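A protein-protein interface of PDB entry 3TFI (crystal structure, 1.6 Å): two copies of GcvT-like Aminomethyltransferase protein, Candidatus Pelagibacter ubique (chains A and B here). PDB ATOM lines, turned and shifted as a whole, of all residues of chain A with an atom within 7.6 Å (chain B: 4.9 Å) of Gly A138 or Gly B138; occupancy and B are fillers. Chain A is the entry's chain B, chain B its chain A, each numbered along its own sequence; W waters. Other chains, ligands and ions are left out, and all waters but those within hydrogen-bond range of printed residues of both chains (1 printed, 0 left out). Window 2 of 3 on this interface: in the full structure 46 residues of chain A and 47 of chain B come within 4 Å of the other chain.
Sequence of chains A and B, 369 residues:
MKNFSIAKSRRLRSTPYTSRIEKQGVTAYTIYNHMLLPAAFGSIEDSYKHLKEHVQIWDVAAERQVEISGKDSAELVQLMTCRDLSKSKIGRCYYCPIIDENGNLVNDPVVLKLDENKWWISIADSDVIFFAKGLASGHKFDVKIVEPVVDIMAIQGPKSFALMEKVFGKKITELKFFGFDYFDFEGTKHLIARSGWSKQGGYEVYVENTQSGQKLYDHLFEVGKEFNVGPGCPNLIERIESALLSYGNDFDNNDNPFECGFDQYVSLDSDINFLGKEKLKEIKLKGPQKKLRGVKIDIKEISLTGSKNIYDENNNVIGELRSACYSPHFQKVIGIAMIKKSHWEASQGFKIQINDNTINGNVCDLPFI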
ATOM      1  N   LEU A  79      -8.649 -24.252  -4.741  1.00  0.00           N
ATOM      2  CA  LEU A  79      -7.844 -23.365  -5.597  1.00  0.00           C
ATOM      3  C   LEU A  79      -7.393 -24.030  -6.871  1.00  0.00           C
ATOM      4  O   LEU A  79      -7.257 -23.380  -7.915  1.00  0.00           O
ATOM      5  CB  LEU A  79      -6.620 -22.873  -4.836  1.00  0.00           C
ATOM      6  CG  LEU A  79      -5.741 -21.806  -5.552  1.00  0.00           C
ATOM      7  CD1 LEU A  79      -6.560 -20.538  -5.878  1.00  0.00           C
ATOM      8  CD2 LEU A  79      -4.472 -21.454  -4.744  1.00  0.00           C
ATOM      9  N   ALA A 132       0.570 -28.351  -6.347  1.00  0.00           N
ATOM     10  CA  ALA A 132       0.116 -28.063  -4.986  1.00  0.00           C
ATOM     11  C   ALA A 132       1.180 -27.386  -4.124  1.00  0.00           C
ATOM     12  O   ALA A 132       0.919 -26.377  -3.430  1.00  0.00           O
ATOM     13  CB  ALA A 132      -0.458 -29.327  -4.306  1.00  0.00           C
ATOM     14  N   LYS A 133       2.373 -27.955  -4.105  1.00  0.00           N
ATOM     15  CA  LYS A 133       3.497 -27.426  -3.310  1.00  0.00           C
ATOM     16  C   LYS A 133       3.846 -26.014  -3.772  1.00  0.00           C
ATOM     17  O   LYS A 133       4.107 -25.155  -2.954  1.00  0.00           O
ATOM     18  CB  LYS A 133       4.711 -28.356  -3.432  1.00  0.00           C
ATOM     19  CG  LYS A 133       4.606 -29.609  -2.590  1.00  0.00           C
ATOM     20  CD  LYS A 133       5.769 -30.584  -2.895  1.00  0.00           C
ATOM     21  CE  LYS A 133       5.803 -31.797  -2.016  1.00  0.00           C
ATOM     22  NZ  LYS A 133       6.674 -31.643  -0.862  1.00  0.00           N
ATOM     23  N   GLY A 134       3.820 -25.789  -5.077  1.00  0.00           N
ATOM     24  CA  GLY A 134       4.132 -24.438  -5.628  1.00  0.00           C
ATOM     25  C   GLY A 134       3.133 -23.447  -5.122  1.00  0.00           C
ATOM     26  O   GLY A 134       3.505 -22.367  -4.652  1.00  0.00           O
ATOM     27  N   LEU A 135       1.860 -23.787  -5.288  1.00  0.00           N
ATOM     28  CA  LEU A 135       0.775 -22.900  -4.831  1.00  0.00           C
ATOM     29  C   LEU A 135       0.864 -22.626  -3.333  1.00  0.00           C
ATOM     30  O   LEU A 135       0.699 -21.455  -2.884  1.00  0.00           O
ATOM     31  CB  LEU A 135      -0.598 -23.494  -5.199  1.00  0.00           C
ATOM     32  CG  LEU A 135      -1.049 -23.453  -6.669  1.00  0.00           C
ATOM     33  CD1 LEU A 135      -2.313 -24.360  -6.982  1.00  0.00           C
ATOM     34  CD2 LEU A 135      -1.238 -21.959  -7.191  1.00  0.00           C
ATOM     35  N   ALA A 136       1.107 -23.648  -2.537  1.00  0.00           N
ATOM     36  CA  ALA A 136       1.160 -23.530  -1.081  1.00  0.00           C
ATOM     37  C   ALA A 136       2.270 -22.601  -0.621  1.00  0.00           C
ATOM     38  O   ALA A 136       2.102 -21.840   0.337  1.00  0.00           O
ATOM     39  CB  ALA A 136       1.344 -24.949  -0.479  1.00  0.00           C
ATOM     40  N   SER A 137       3.411 -22.658  -1.325  1.00  0.00           N
ATOM     41  CA  SER A 137       4.557 -21.827  -1.031  1.00  0.00           C
ATOM     42  C   SER A 137       4.259 -20.372  -1.261  1.00  0.00           C
ATOM     43  O   SER A 137       4.568 -19.540  -0.400  1.00  0.00           O
ATOM     44  CB  SER A 137       5.744 -22.247  -1.930  1.00  0.00           C
ATOM     45  OG  SER A 137       6.798 -21.346  -1.760  1.00  0.00           O
ATOM     46  N   GLY A 138       3.616 -20.053  -2.385  1.00  0.00           N
ATOM     47  CA  GLY A 138       3.325 -18.645  -2.687  1.00  0.00           C
ATOM     48  C   GLY A 138       2.250 -18.018  -1.788  1.00  0.00           C
ATOM     49  O   GLY A 138       2.329 -16.850  -1.362  1.00  0.00           O
ATOM     50  N   HIS A 139       1.258 -18.831  -1.449  1.00  0.00           N
ATOM     51  CA  HIS A 139       0.145 -18.394  -0.548  1.00  0.00           C
ATOM     52  C   HIS A 139       0.483 -18.507   0.912  1.00  0.00           C
ATOM     53  O   HIS A 139      -0.314 -18.029   1.765  1.00  0.00           O
ATOM     54  CB  HIS A 139      -1.100 -19.209  -0.818  1.00  0.00           C
ATOM     55  CG  HIS A 139      -1.782 -18.842  -2.083  1.00  0.00           C
ATOM     56  ND1 HIS A 139      -2.617 -17.747  -2.170  1.00  0.00           N
ATOM     57  CD2 HIS A 139      -1.684 -19.343  -3.345  1.00  0.00           C
ATOM     58  CE1 HIS A 139      -3.057 -17.627  -3.404  1.00  0.00           C
ATOM     59  NE2 HIS A 139      -2.482 -18.549  -4.144  1.00  0.00           N
ATOM     60  N   LYS A 140       1.624 -19.135   1.221  1.00  0.00           N
ATOM     61  CA  LYS A 140       2.034 -19.432   2.590  1.00  0.00           C
ATOM     62  C   LYS A 140       0.925 -20.199   3.325  1.00  0.00           C
ATOM     63  O   LYS A 140       0.638 -19.964   4.535  1.00  0.00           O
ATOM     64  CB  LYS A 140       2.489 -18.161   3.301  1.00  0.00           C
ATOM     65  CG  LYS A 140       3.494 -17.340   2.473  1.00  0.00           C
ATOM     66  CD  LYS A 140       4.028 -16.117   3.244  1.00  0.00           C
ATOM     67  CE  LYS A 140       5.345 -15.604   2.601  1.00  0.00           C
ATOM     68  NZ  LYS A 140       5.930 -14.405   3.273  1.00  0.00           N
ATOM     69  N   PHE A 141       0.281 -21.128   2.624  1.00  0.00           N
ATOM     70  CA  PHE A 141      -0.770 -21.912   3.257  1.00  0.00           C
ATOM     71  C   PHE A 141      -0.219 -22.779   4.384  1.00  0.00           C
ATOM     72  O   PHE A 141       0.875 -23.397   4.292  1.00  0.00           O
ATOM     73  CB  PHE A 141      -1.469 -22.834   2.252  1.00  0.00           C
ATOM     74  CG  PHE A 141      -2.430 -22.144   1.323  1.00  0.00           C
ATOM     75  CD1 PHE A 141      -3.224 -21.065   1.777  1.00  0.00           C
ATOM     76  CD2 PHE A 141      -2.512 -22.497   0.008  1.00  0.00           C
ATOM     77  CE1 PHE A 141      -4.171 -20.491   0.937  1.00  0.00           C
ATOM     78  CE2 PHE A 141      -3.410 -21.911  -0.862  1.00  0.00           C
ATOM     79  CZ  PHE A 141      -4.251 -20.881  -0.412  1.00  0.00           C
ATOM     80  N   LEU A 275      -7.784 -21.133 -10.057  1.00  0.00           N
ATOM     81  CA  LEU A 275      -6.978 -20.621 -11.237  1.00  0.00           C
ATOM     82  C   LEU A 275      -7.713 -20.550 -12.538  1.00  0.00           C
ATOM     83  O   LEU A 275      -8.510 -21.420 -12.891  1.00  0.00           O
ATOM     84  CB  LEU A 275      -5.693 -21.482 -11.488  1.00  0.00           C
ATOM     85  CG  LEU A 275      -4.463 -21.049 -10.721  1.00  0.00           C
ATOM     86  CD1 LEU A 275      -4.695 -21.447  -9.326  1.00  0.00           C
ATOM     87  CD2 LEU A 275      -3.105 -21.558 -11.189  1.00  0.00           C
ATOM     88  N   GLY B 134       2.688 -23.416 -10.350  1.00  0.00           N
ATOM     89  CA  GLY B 134       2.133 -23.233  -9.002  1.00  0.00           C
ATOM     90  C   GLY B 134       2.796 -22.077  -8.267  1.00  0.00           C
ATOM     91  O   GLY B 134       2.100 -21.248  -7.649  1.00  0.00           O
ATOM     92  N   LEU B 135       4.126 -22.030  -8.308  1.00  0.00           N
ATOM     93  CA  LEU B 135       4.917 -20.945  -7.699  1.00  0.00           C
ATOM     94  C   LEU B 135       4.567 -19.604  -8.263  1.00  0.00           C
ATOM     95  O   LEU B 135       4.366 -18.593  -7.501  1.00  0.00           O
ATOM     96  CB  LEU B 135       6.429 -21.189  -7.774  1.00  0.00           C
ATOM     97  CG  LEU B 135       7.001 -22.305  -6.868  1.00  0.00           C
ATOM     98  CD1 LEU B 135       8.434 -22.661  -7.326  1.00  0.00           C
ATOM     99  CD2 LEU B 135       6.981 -21.991  -5.374  1.00  0.00           C
ATOM    100  N   ALA B 136       4.472 -19.537  -9.594  1.00  0.00           N
ATOM    101  CA  ALA B 136       4.230 -18.260 -10.223  1.00  0.00           C
ATOM    102  C   ALA B 136       2.850 -17.737  -9.848  1.00  0.00           C
ATOM    103  O   ALA B 136       2.682 -16.514  -9.597  1.00  0.00           O
ATOM    104  CB  ALA B 136       4.392 -18.416 -11.795  1.00  0.00           C
ATOM    105  N   SER B 137       1.856 -18.612  -9.789  1.00  0.00           N
ATOM    106  CA  SER B 137       0.528 -18.194  -9.420  1.00  0.00           C
ATOM    107  C   SER B 137       0.539 -17.735  -7.948  1.00  0.00           C
ATOM    108  O   SER B 137      -0.007 -16.656  -7.603  1.00  0.00           O
ATOM    109  CB  SER B 137      -0.467 -19.325  -9.623  1.00  0.00           C
ATOM    110  OG  SER B 137      -1.774 -19.007  -9.170  1.00  0.00           O
ATOM    111  N   GLY B 138       1.141 -18.520  -7.053  1.00  0.00           N
ATOM    112  CA  GLY B 138       1.085 -18.172  -5.655  1.00  0.00           C
ATOM    113  C   GLY B 138       1.851 -16.922  -5.280  1.00  0.00           C
ATOM    114  O   GLY B 138       1.442 -16.137  -4.408  1.00  0.00           O
ATOM    115  N   HIS B 139       3.000 -16.749  -5.925  1.00  0.00           N
ATOM    116  CA  HIS B 139       3.866 -15.579  -5.768  1.00  0.00           C
ATOM    117  C   HIS B 139       3.454 -14.390  -6.651  1.00  0.00           C
ATOM    118  O   HIS B 139       4.034 -13.292  -6.488  1.00  0.00           O
ATOM    119  CB  HIS B 139       5.329 -15.973  -5.983  1.00  0.00           C
ATOM    120  CG  HIS B 139       5.934 -16.771  -4.850  1.00  0.00           C
ATOM    121  ND1 HIS B 139       5.873 -18.144  -4.735  1.00  0.00           N
ATOM    122  CD2 HIS B 139       6.652 -16.346  -3.789  1.00  0.00           C
ATOM    123  CE1 HIS B 139       6.500 -18.521  -3.627  1.00  0.00           C
ATOM    124  NE2 HIS B 139       7.004 -17.447  -3.060  1.00  0.00           N
ATOM    125  N   LYS B 140       2.399 -14.531  -7.452  1.00  0.00           N
ATOM    126  CA  LYS B 140       1.913 -13.490  -8.389  1.00  0.00           C
ATOM    127  C   LYS B 140       3.031 -12.911  -9.271  1.00  0.00           C
ATOM    128  O   LYS B 140       3.089 -11.697  -9.550  1.00  0.00           O
ATOM    129  CB  LYS B 140       1.049 -12.390  -7.701  1.00  0.00           C
ATOM    130  CG  LYS B 140      -0.317 -12.953  -7.196  1.00  0.00           C
ATOM    131  CD  LYS B 140      -1.229 -11.926  -6.489  1.00  0.00           C
ATOM    132  CE  LYS B 140      -2.242 -12.594  -5.542  1.00  0.00           C
ATOM    133  NZ  LYS B 140      -1.755 -12.573  -4.089  1.00  0.00           N
HETATM  134  O   HOH W   1      -3.230 -18.641  -6.858  1.00  0.00           O
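N of Leu A135 lies close to O of Gly B134 (3.5 Å).
O of Gly A134 lies close to O of Gly B134 (3.5 Å).
The backbone carbonyl oxygen (O) of Gly B138 sits close to the backbone carbonyl oxygen (O) of Gly A138 (3.3 Å).
ND1 of His B139 lies close to O of Leu B135, at 3.2 Å.
The backbone carbonyl oxygen (O) of Leu A79 is in hydrogen-bond range of the backbone NH (N) of Leu A275 (3.1 Å).
Among the printed residues, pairs that only touch across the chains: Gly A134 with Leu B135 (3.6 Å), Leu A135 with Ser B137 (3.6 Å), Ser A137 with Leu B135 (3.7 Å), Ser A137 with His B139 (3.4 Å), Gly A138 with His B139 (3.3 Å), His A139 with Gly B138 (3.8 Å) and Leu A275 with Ser B137 (3.5 Å).
Ala A136 touches none of the printed residues of chain B.
Gly A138 touches just these residues of chain B: Gly B138 (3.3 Å) and His B139 (3.3 Å).
Of the printed residues of chain B, His A139 touches Gly B138.
Of the printed residues of chain A, Ser B137 touches Leu A135 and Leu A275.
Printed residues of chain A within 4 Å of His B139: Ser A137 (3.4 Å) and Gly A138 (3.3 Å).
The nearest printed residue of chain B that does not touch Gly A138 is Leu B135 (4.9 Å).
The nearest residue of chain A that does not touch Gly B138 is Leu A135 (4.2 Å).
The nearest printed residue of chain B that does not touch Ser A137 is Gly B138 (5.8 Å).
Of the 7 printed residues of chain B, 5 touch a printed residue of chain A.
Printed residues of chain B that touch a printed residue of chain A: Gly B134, Leu B135, Ser B137, Gly B138 and His B139.
Printed residues of chain A that touch a printed residue of chain B: Gly A134, Leu A135, Ser A137, Gly A138, His A139 and Leu A275.
Hydrophobic or aromatic side chains of chain A that line the printed part of chain B: Leu A135, His A139 and Leu A275.
Among the printed residues, 10 pairs touch across the chains.
Gly A134 touches Leu B135, and with the chains exchanged Leu A135 touches Gly B134.
Ser A137 touches His B139, but with the chains exchanged His A139 does not touch Ser B137 (4.7 Å).
Gly A138 touches its own counterpart, Gly B138.
Gly A138 touches His B139, and with the chains exchanged His A139 touches Gly B138.
Positions printed for both chains: 134, 135, 136, 137, 138, 139 and 140.
Of the 10 pairs that touch across the chains among the printed residues, 8 have their exchanged pair printed and touching as well.
Water W1 bridges the side-chain hydroxyl (OG) of Ser B137 (2.8 Å) and a ring nitrogen (NE2) of His A139 (2.8 Å).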
